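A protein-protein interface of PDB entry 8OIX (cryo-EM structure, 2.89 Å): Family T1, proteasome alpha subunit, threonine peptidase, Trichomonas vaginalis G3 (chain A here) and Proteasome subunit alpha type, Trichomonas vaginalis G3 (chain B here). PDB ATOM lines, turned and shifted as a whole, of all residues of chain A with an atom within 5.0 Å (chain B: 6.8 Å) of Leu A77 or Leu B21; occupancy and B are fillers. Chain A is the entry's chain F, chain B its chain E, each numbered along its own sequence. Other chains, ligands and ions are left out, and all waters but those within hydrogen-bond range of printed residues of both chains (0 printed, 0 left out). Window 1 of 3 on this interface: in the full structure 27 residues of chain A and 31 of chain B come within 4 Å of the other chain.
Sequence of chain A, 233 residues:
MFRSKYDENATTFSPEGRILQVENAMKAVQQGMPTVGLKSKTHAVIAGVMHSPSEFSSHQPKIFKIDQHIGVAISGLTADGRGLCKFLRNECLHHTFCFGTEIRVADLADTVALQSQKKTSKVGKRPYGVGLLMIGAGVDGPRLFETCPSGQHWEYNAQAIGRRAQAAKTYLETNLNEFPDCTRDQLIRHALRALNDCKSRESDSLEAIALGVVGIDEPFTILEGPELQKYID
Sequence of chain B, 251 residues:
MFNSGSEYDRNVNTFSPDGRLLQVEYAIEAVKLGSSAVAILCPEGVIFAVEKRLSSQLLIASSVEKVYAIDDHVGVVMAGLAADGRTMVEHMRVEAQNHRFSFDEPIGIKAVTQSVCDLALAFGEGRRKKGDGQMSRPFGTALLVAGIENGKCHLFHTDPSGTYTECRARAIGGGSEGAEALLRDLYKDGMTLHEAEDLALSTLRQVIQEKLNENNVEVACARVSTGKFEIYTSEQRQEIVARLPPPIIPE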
ATOM      1  N   ALA A  28     -25.693   0.533   0.883  1.00  0.00           N
ATOM      2  CA  ALA A  28     -26.736  -0.245   0.223  1.00  0.00           C
ATOM      3  C   ALA A  28     -27.874   0.648  -0.242  1.00  0.00           C
ATOM      4  O   ALA A  28     -28.474   0.401  -1.295  1.00  0.00           O
ATOM      5  CB  ALA A  28     -27.269  -1.322   1.167  1.00  0.00           C
ATOM      6  N   ILE A  74     -38.736   4.154  -1.958  1.00  0.00           N
ATOM      7  CA  ILE A  74     -37.678   3.341  -1.374  1.00  0.00           C
ATOM      8  C   ILE A  74     -36.435   3.421  -2.249  1.00  0.00           C
ATOM      9  O   ILE A  74     -36.511   3.596  -3.469  1.00  0.00           O
ATOM     10  CB  ILE A  74     -38.149   1.884  -1.183  1.00  0.00           C
ATOM     11  CG1 ILE A  74     -38.138   1.132  -2.513  1.00  0.00           C
ATOM     12  CG2 ILE A  74     -39.539   1.852  -0.575  1.00  0.00           C
ATOM     13  CD1 ILE A  74     -38.634  -0.286  -2.410  1.00  0.00           C
ATOM     14  N   SER A  75     -35.269   3.322  -1.610  1.00  0.00           N
ATOM     15  CA  SER A  75     -33.989   3.260  -2.311  1.00  0.00           C
ATOM     16  C   SER A  75     -33.107   2.265  -1.572  1.00  0.00           C
ATOM     17  O   SER A  75     -32.689   2.530  -0.442  1.00  0.00           O
ATOM     18  CB  SER A  75     -33.323   4.633  -2.381  1.00  0.00           C
ATOM     19  OG  SER A  75     -32.132   4.582  -3.146  1.00  0.00           O
ATOM     20  N   GLY A  76     -32.831   1.126  -2.197  1.00  0.00           N
ATOM     21  CA  GLY A  76     -32.070   0.083  -1.540  1.00  0.00           C
ATOM     22  C   GLY A  76     -32.759  -1.257  -1.655  1.00  0.00           C
ATOM     23  O   GLY A  76     -33.441  -1.517  -2.650  1.00  0.00           O
ATOM     24  N   LEU A  77     -32.580  -2.123  -0.657  1.00  0.00           N
ATOM     25  CA  LEU A  77     -33.244  -3.421  -0.667  1.00  0.00           C
ATOM     26  C   LEU A  77     -34.751  -3.219  -0.722  1.00  0.00           C
ATOM     27  O   LEU A  77     -35.353  -2.737   0.243  1.00  0.00           O
ATOM     28  CB  LEU A  77     -32.855  -4.237   0.567  1.00  0.00           C
ATOM     29  CG  LEU A  77     -31.407  -4.721   0.641  1.00  0.00           C
ATOM     30  CD1 LEU A  77     -31.123  -5.342   1.998  1.00  0.00           C
ATOM     31  CD2 LEU A  77     -31.115  -5.709  -0.475  1.00  0.00           C
ATOM     32  N   THR A  78     -35.367  -3.577  -1.851  1.00  0.00           N
ATOM     33  CA  THR A  78     -36.803  -3.365  -2.000  1.00  0.00           C
ATOM     34  C   THR A  78     -37.605  -4.222  -1.033  1.00  0.00           C
ATOM     35  O   THR A  78     -38.728  -3.858  -0.677  1.00  0.00           O
ATOM     36  CB  THR A  78     -37.245  -3.637  -3.435  1.00  0.00           C
ATOM     37  OG1 THR A  78     -37.140  -5.035  -3.705  1.00  0.00           O
ATOM     38  CG2 THR A  78     -36.373  -2.867  -4.417  1.00  0.00           C
ATOM     39  N   ALA A  79     -37.074  -5.377  -0.630  1.00  0.00           N
ATOM     40  CA  ALA A  79     -37.754  -6.185   0.377  1.00  0.00           C
ATOM     41  C   ALA A  79     -37.787  -5.466   1.722  1.00  0.00           C
ATOM     42  O   ALA A  79     -38.820  -5.445   2.403  1.00  0.00           O
ATOM     43  CB  ALA A  79     -37.077  -7.547   0.502  1.00  0.00           C
ATOM     44  N   ASP A  80     -36.659  -4.876   2.125  1.00  0.00           N
ATOM     45  CA  ASP A  80     -36.651  -4.052   3.328  1.00  0.00           C
ATOM     46  C   ASP A  80     -37.560  -2.843   3.164  1.00  0.00           C
ATOM     47  O   ASP A  80     -38.211  -2.409   4.120  1.00  0.00           O
ATOM     48  CB  ASP A  80     -35.227  -3.611   3.661  1.00  0.00           C
ATOM     49  CG  ASP A  80     -34.425  -4.698   4.339  1.00  0.00           C
ATOM     50  OD1 ASP A  80     -35.020  -5.734   4.703  1.00  0.00           O
ATOM     51  OD2 ASP A  80     -33.201  -4.518   4.510  1.00  0.00           O
ATOM     52  N   GLY A  81     -37.608  -2.280   1.955  1.00  0.00           N
ATOM     53  CA  GLY A  81     -38.531  -1.188   1.700  1.00  0.00           C
ATOM     54  C   GLY A  81     -39.978  -1.601   1.880  1.00  0.00           C
ATOM     55  O   GLY A  81     -40.781  -0.849   2.428  1.00  0.00           O
ATOM     56  N   ARG A 126     -30.266  -6.421  11.753  1.00  0.00           N
ATOM     57  CA  ARG A 126     -29.548  -5.626  10.781  1.00  0.00           C
ATOM     58  C   ARG A 126     -30.300  -4.333  10.501  1.00  0.00           C
ATOM     59  O   ARG A 126     -31.534  -4.301  10.551  1.00  0.00           O
ATOM     60  CB  ARG A 126     -29.358  -6.391   9.467  1.00  0.00           C
ATOM     61  CG  ARG A 126     -30.658  -6.861   8.851  1.00  0.00           C
ATOM     62  CD  ARG A 126     -30.513  -7.145   7.371  1.00  0.00           C
ATOM     63  NE  ARG A 126     -31.813  -7.163   6.715  1.00  0.00           N
ATOM     64  CZ  ARG A 126     -32.609  -8.221   6.662  1.00  0.00           C
ATOM     65  NH1 ARG A 126     -32.256  -9.379   7.196  1.00  0.00           N
ATOM     66  NH2 ARG A 126     -33.791  -8.113   6.064  1.00  0.00           N
ATOM     67  N   GLY A 129     -31.813  -2.105   4.894  1.00  0.00           N
ATOM     68  CA  GLY A 129     -30.961  -1.715   3.790  1.00  0.00           C
ATOM     69  C   GLY A 129     -31.668  -0.837   2.781  1.00  0.00           C
ATOM     70  O   GLY A 129     -31.409  -0.925   1.577  1.00  0.00           O
ATOM     71  N   VAL A 130     -32.565   0.017   3.264  1.00  0.00           N
ATOM     72  CA  VAL A 130     -33.399   0.853   2.410  1.00  0.00           C
ATOM     73  C   VAL A 130     -33.538   2.227   3.051  1.00  0.00           C
ATOM     74  O   VAL A 130     -33.688   2.349   4.271  1.00  0.00           O
ATOM     75  CB  VAL A 130     -34.776   0.202   2.159  1.00  0.00           C
ATOM     76  CG1 VAL A 130     -35.531   0.021   3.461  1.00  0.00           C
ATOM     77  CG2 VAL A 130     -35.583   1.030   1.181  1.00  0.00           C
ATOM     78  N   VAL B  12     -25.460 -13.737   9.740  1.00  0.00           N
ATOM     79  CA  VAL B  12     -26.227 -13.870   8.502  1.00  0.00           C
ATOM     80  C   VAL B  12     -26.675 -12.506   7.990  1.00  0.00           C
ATOM     81  O   VAL B  12     -26.593 -12.217   6.789  1.00  0.00           O
ATOM     82  CB  VAL B  12     -27.420 -14.825   8.697  1.00  0.00           C
ATOM     83  CG1 VAL B  12     -26.928 -16.228   8.966  1.00  0.00           C
ATOM     84  CG2 VAL B  12     -28.328 -14.356   9.815  1.00  0.00           C
ATOM     85  N   ASN B  13     -27.153 -11.647   8.884  1.00  0.00           N
ATOM     86  CA  ASN B  13     -27.699 -10.353   8.488  1.00  0.00           C
ATOM     87  C   ASN B  13     -26.625  -9.273   8.608  1.00  0.00           C
ATOM     88  O   ASN B  13     -26.706  -8.341   9.408  1.00  0.00           O
ATOM     89  CB  ASN B  13     -28.939 -10.030   9.318  1.00  0.00           C
ATOM     90  CG  ASN B  13     -28.734 -10.275  10.801  1.00  0.00           C
ATOM     91  OD1 ASN B  13     -27.625 -10.150  11.320  1.00  0.00           O
ATOM     92  ND2 ASN B  13     -29.809 -10.636  11.491  1.00  0.00           N
ATOM     93  N   THR B  14     -25.602  -9.417   7.768  1.00  0.00           N
ATOM     94  CA  THR B  14     -24.483  -8.488   7.719  1.00  0.00           C
ATOM     95  C   THR B  14     -24.396  -7.888   6.324  1.00  0.00           C
ATOM     96  O   THR B  14     -24.688  -8.558   5.327  1.00  0.00           O
ATOM     97  CB  THR B  14     -23.153  -9.169   8.084  1.00  0.00           C
ATOM     98  OG1 THR B  14     -22.124  -8.178   8.190  1.00  0.00           O
ATOM     99  CG2 THR B  14     -22.744 -10.177   7.023  1.00  0.00           C
ATOM    100  N   PHE B  15     -24.028  -6.615   6.261  1.00  0.00           N
ATOM    101  CA  PHE B  15     -23.900  -5.902   5.000  1.00  0.00           C
ATOM    102  C   PHE B  15     -22.428  -5.791   4.630  1.00  0.00           C
ATOM    103  O   PHE B  15     -21.602  -5.405   5.462  1.00  0.00           O
ATOM    104  CB  PHE B  15     -24.529  -4.512   5.093  1.00  0.00           C
ATOM    105  CG  PHE B  15     -26.027  -4.519   5.080  1.00  0.00           C
ATOM    106  CD1 PHE B  15     -26.722  -4.575   3.886  1.00  0.00           C
ATOM    107  CD2 PHE B  15     -26.740  -4.461   6.263  1.00  0.00           C
ATOM    108  CE1 PHE B  15     -28.101  -4.576   3.871  1.00  0.00           C
ATOM    109  CE2 PHE B  15     -28.119  -4.464   6.254  1.00  0.00           C
ATOM    110  CZ  PHE B  15     -28.800  -4.521   5.057  1.00  0.00           C
ATOM    111  N   SER B  16     -22.108  -6.129   3.386  1.00  0.00           N
ATOM    112  CA  SER B  16     -20.758  -5.956   2.889  1.00  0.00           C
ATOM    113  C   SER B  16     -20.442  -4.469   2.751  1.00  0.00           C
ATOM    114  O   SER B  16     -21.348  -3.643   2.627  1.00  0.00           O
ATOM    115  CB  SER B  16     -20.595  -6.656   1.544  1.00  0.00           C
ATOM    116  OG  SER B  16     -21.231  -5.924   0.511  1.00  0.00           O
ATOM    117  N   GLY B  19     -22.405  -2.598   0.456  1.00  0.00           N
ATOM    118  CA  GLY B  19     -23.836  -2.485   0.671  1.00  0.00           C
ATOM    119  C   GLY B  19     -24.658  -3.639   0.140  1.00  0.00           C
ATOM    120  O   GLY B  19     -25.707  -3.414  -0.477  1.00  0.00           O
ATOM    121  N   ARG B  20     -24.199  -4.870   0.338  1.00  0.00           N
ATOM    122  CA  ARG B  20     -24.963  -6.052  -0.030  1.00  0.00           C
ATOM    123  C   ARG B  20     -25.078  -6.982   1.167  1.00  0.00           C
ATOM    124  O   ARG B  20     -24.112  -7.173   1.910  1.00  0.00           O
ATOM    125  CB  ARG B  20     -24.321  -6.802  -1.203  1.00  0.00           C
ATOM    126  CG  ARG B  20     -24.341  -6.053  -2.521  1.00  0.00           C
ATOM    127  CD  ARG B  20     -23.843  -6.944  -3.647  1.00  0.00           C
ATOM    128  NE  ARG B  20     -22.599  -7.616  -3.292  1.00  0.00           N
ATOM    129  CZ  ARG B  20     -21.391  -7.105  -3.490  1.00  0.00           C
ATOM    130  NH1 ARG B  20     -21.225  -5.932  -4.077  1.00  0.00           N
ATOM    131  NH2 ARG B  20     -20.324  -7.793  -3.095  1.00  0.00           N
ATOM    132  N   LEU B  21     -26.264  -7.557   1.351  1.00  0.00           N
ATOM    133  CA  LEU B  21     -26.456  -8.603   2.348  1.00  0.00           C
ATOM    134  C   LEU B  21     -25.726  -9.856   1.881  1.00  0.00           C
ATOM    135  O   LEU B  21     -26.124 -10.479   0.893  1.00  0.00           O
ATOM    136  CB  LEU B  21     -27.941  -8.878   2.557  1.00  0.00           C
ATOM    137  CG  LEU B  21     -28.643  -8.125   3.687  1.00  0.00           C
ATOM    138  CD1 LEU B  21     -30.110  -8.507   3.746  1.00  0.00           C
ATOM    139  CD2 LEU B  21     -27.965  -8.407   5.014  1.00  0.00           C
ATOM    140  N   LEU B  22     -24.648 -10.216   2.581  1.00  0.00           N
ATOM    141  CA  LEU B  22     -23.782 -11.290   2.104  1.00  0.00           C
ATOM    142  C   LEU B  22     -24.536 -12.607   1.975  1.00  0.00           C
ATOM    143  O   LEU B  22     -24.384 -13.319   0.978  1.00  0.00           O
ATOM    144  CB  LEU B  22     -22.584 -11.446   3.036  1.00  0.00           C
ATOM    145  CG  LEU B  22     -21.556 -10.319   2.946  1.00  0.00           C
ATOM    146  CD1 LEU B  22     -20.472 -10.498   3.991  1.00  0.00           C
ATOM    147  CD2 LEU B  22     -20.959 -10.272   1.550  1.00  0.00           C
ATOM    148  N   GLN B  23     -25.369 -12.941   2.963  1.00  0.00           N
ATOM    149  CA  GLN B  23     -26.164 -14.160   2.862  1.00  0.00           C
ATOM    150  C   GLN B  23     -27.130 -14.091   1.690  1.00  0.00           C
ATOM    151  O   GLN B  23     -27.400 -15.105   1.041  1.00  0.00           O
ATOM    152  CB  GLN B  23     -26.914 -14.417   4.166  1.00  0.00           C
ATOM    153  CG  GLN B  23     -26.049 -15.020   5.249  1.00  0.00           C
ATOM    154  CD  GLN B  23     -25.475 -16.366   4.861  1.00  0.00           C
ATOM    155  OE1 GLN B  23     -26.146 -17.392   4.968  1.00  0.00           O
ATOM    156  NE2 GLN B  23     -24.225 -16.370   4.414  1.00  0.00           N
ATOM    157  N   VAL B  24     -27.666 -12.905   1.406  1.00  0.00           N
ATOM    158  CA  VAL B  24     -28.566 -12.759   0.268  1.00  0.00           C
ATOM    159  C   VAL B  24     -27.831 -13.022  -1.040  1.00  0.00           C
ATOM    160  O   VAL B  24     -28.327 -13.745  -1.911  1.00  0.00           O
ATOM    161  CB  VAL B  24     -29.210 -11.365   0.283  1.00  0.00           C
ATOM    162  CG1 VAL B  24     -29.685 -10.998  -1.097  1.00  0.00           C
ATOM    163  CG2 VAL B  24     -30.360 -11.338   1.265  1.00  0.00           C
ATOM    164  N   GLU B  25     -26.629 -12.464  -1.194  1.00  0.00           N
ATOM    165  CA  GLU B  25     -25.863 -12.704  -2.412  1.00  0.00           C
ATOM    166  C   GLU B  25     -25.471 -14.169  -2.532  1.00  0.00           C
ATOM    167  O   GLU B  25     -25.476 -14.736  -3.631  1.00  0.00           O
ATOM    168  CB  GLU B  25     -24.628 -11.805  -2.439  1.00  0.00           C
ATOM    169  CG  GLU B  25     -24.918 -10.330  -2.179  1.00  0.00           C
ATOM    170  CD  GLU B  25     -26.105  -9.797  -2.968  1.00  0.00           C
ATOM    171  OE1 GLU B  25     -26.292 -10.199  -4.136  1.00  0.00           O
ATOM    172  OE2 GLU B  25     -26.857  -8.970  -2.412  1.00  0.00           O
ATOM    173  N   TYR B  26     -25.140 -14.803  -1.409  1.00  0.00           N
ATOM    174  CA  TYR B  26     -24.772 -16.213  -1.448  1.00  0.00           C
ATOM    175  C   TYR B  26     -25.974 -17.095  -1.769  1.00  0.00           C
ATOM    176  O   TYR B  26     -25.828 -18.121  -2.440  1.00  0.00           O
ATOM    177  CB  TYR B  26     -24.143 -16.619  -0.117  1.00  0.00           C
ATOM    178  CG  TYR B  26     -22.957 -15.773   0.311  1.00  0.00           C
ATOM    179  CD1 TYR B  26     -22.282 -14.964  -0.595  1.00  0.00           C
ATOM    180  CD2 TYR B  26     -22.525 -15.778   1.631  1.00  0.00           C
ATOM    181  CE1 TYR B  26     -21.209 -14.190  -0.202  1.00  0.00           C
ATOM    182  CE2 TYR B  26     -21.451 -15.008   2.033  1.00  0.00           C
ATOM    183  CZ  TYR B  26     -20.797 -14.216   1.113  1.00  0.00           C
ATOM    184  OH  TYR B  26     -19.727 -13.447   1.509  1.00  0.00           O
ATOM    185  N   ALA B  27     -27.166 -16.709  -1.318  1.00  0.00           N
ATOM    186  CA  ALA B  27     -28.380 -17.411  -1.721  1.00  0.00           C
ATOM    187  C   ALA B  27     -28.674 -17.203  -3.204  1.00  0.00           C
ATOM    188  O   ALA B  27     -29.181 -18.109  -3.874  1.00  0.00           O
ATOM    189  CB  ALA B  27     -29.553 -16.956  -0.857  1.00  0.00           C
ATOM    190  N   LEU B 121     -37.158 -12.592   3.227  1.00  0.00           N
ATOM    191  CA  LEU B 121     -36.101 -11.828   3.874  1.00  0.00           C
ATOM    192  C   LEU B 121     -36.295 -11.715   5.382  1.00  0.00           C
ATOM    193  O   LEU B 121     -35.636 -10.893   6.025  1.00  0.00           O
ATOM    194  CB  LEU B 121     -35.995 -10.437   3.245  1.00  0.00           C
ATOM    195  CG  LEU B 121     -34.606  -9.799   3.330  1.00  0.00           C
ATOM    196  CD1 LEU B 121     -33.625 -10.593   2.494  1.00  0.00           C
ATOM    197  CD2 LEU B 121     -34.628  -8.351   2.888  1.00  0.00           C
ATOM    198  N   PHE B 123     -35.272 -13.692   7.582  1.00  0.00           N
ATOM    199  CA  PHE B 123     -34.280 -14.517   8.253  1.00  0.00           C
ATOM    200  C   PHE B 123     -33.501 -13.710   9.282  1.00  0.00           C
ATOM    201  O   PHE B 123     -33.246 -12.515   9.108  1.00  0.00           O
ATOM    202  CB  PHE B 123     -33.326 -15.146   7.233  1.00  0.00           C
ATOM    203  CG  PHE B 123     -32.369 -14.173   6.604  1.00  0.00           C
ATOM    204  CD1 PHE B 123     -32.727 -13.467   5.469  1.00  0.00           C
ATOM    205  CD2 PHE B 123     -31.099 -13.987   7.127  1.00  0.00           C
ATOM    206  CE1 PHE B 123     -31.848 -12.580   4.882  1.00  0.00           C
ATOM    207  CE2 PHE B 123     -30.218 -13.101   6.544  1.00  0.00           C
ATOM    208  CZ  PHE B 123     -30.593 -12.397   5.420  1.00  0.00           C
ATOM    209  N   SER B 161     -33.241 -12.269  -2.297  1.00  0.00           N
ATOM    210  CA  SER B 161     -33.200 -10.962  -1.652  1.00  0.00           C
ATOM    211  C   SER B 161     -34.570 -10.499  -1.185  1.00  0.00           C
ATOM    212  O   SER B 161     -34.649  -9.546  -0.403  1.00  0.00           O
ATOM    213  CB  SER B 161     -32.607  -9.920  -2.599  1.00  0.00           C
ATOM    214  OG  SER B 161     -33.449  -9.715  -3.715  1.00  0.00           O
ATOM    215  N   THR B 163     -36.822  -9.293  -3.295  1.00  0.00           N
ATOM    216  CA  THR B 163     -37.372  -8.428  -4.327  1.00  0.00           C
ATOM    217  C   THR B 163     -38.101  -9.266  -5.370  1.00  0.00           C
ATOM    218  O   THR B 163     -37.635 -10.343  -5.757  1.00  0.00           O
ATOM    219  CB  THR B 163     -36.269  -7.585  -4.974  1.00  0.00           C
ATOM    220  OG1 THR B 163     -36.864  -6.576  -5.795  1.00  0.00           O
ATOM    221  CG2 THR B 163     -35.337  -8.421  -5.819  1.00  0.00           C
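The guanidinium group of Arg A126 sits close to the backbone carbonyl oxygen of Leu B121 (3.3 Å).
The side-chain hydroxyl (OG1) of Thr A78 sits at hydrogen-bond distance from the side-chain hydroxyl (OG1) of Thr B163 (2.6 Å).
N of Thr B163 sits close to OG of Ser B161, 3.4 Å away.
The backbone NH (N) of Leu A77 sits at hydrogen-bond distance from the backbone carbonyl oxygen (O) of Gly A129.
OD1 of Asp A80 is in salt-bridge range of NH2 of Arg A126 (3.0 Å).
OD2 of Asp A80 lies within hydrogen-bond range of N of Gly A129.
Among the printed residues, pairs that only touch across the chains: Ala A28 with Gly B19 (3.1 Å), Leu A77 with Phe B15 (3.6 Å), Leu A77 with Leu B21 (3.8 Å), Ala A79 with Leu B121 (3.5 Å), Ala A79 with Ser B161 (3.3 Å), Asp A80 with Leu B121 (3.2 Å), Arg A126 with Asn B13 (3.3 Å), Arg A126 with Phe B15 (3.8 Å), Arg A126 with Leu B21 (3.7 Å), Arg A126 with Phe B123 (3.8 Å) and Gly A129 with Phe B15 (3.8 Å).
Of the printed residues of chain B, Leu A77 touches Phe B15 (3.6 Å) and Leu B21 (3.8 Å).
Printed residues of chain B within 4 Å of Gly A129: Phe B15.
Of the printed residues of chain A, Gly B19 touches Ala A28 (3.1 Å).
Of chain A, only Leu A77 and Arg A126 come within 4 Å of Leu B21.
Printed residues of chain A within 4 Å of Phe B123: Arg A126.
Of the printed residues of chain A, Ser B161 touches Ala A79.
Hydrophobic or aromatic side chains of chain A within 4 Å of the printed part of chain B: Ala A28, Leu A77 and Ala A79.
Of the 18 printed residues of chain B, 8 touch a printed residue of chain A.
Hydrophobic or aromatic side chains of chain B that line the printed part of chain A: Phe B15, Leu B21, Leu B121 and Phe B123.
Along chain B the printed residues that touch a printed residue of chain A span positions 13 to 163.
Among the printed residues, 13 pairs touch across the chains.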
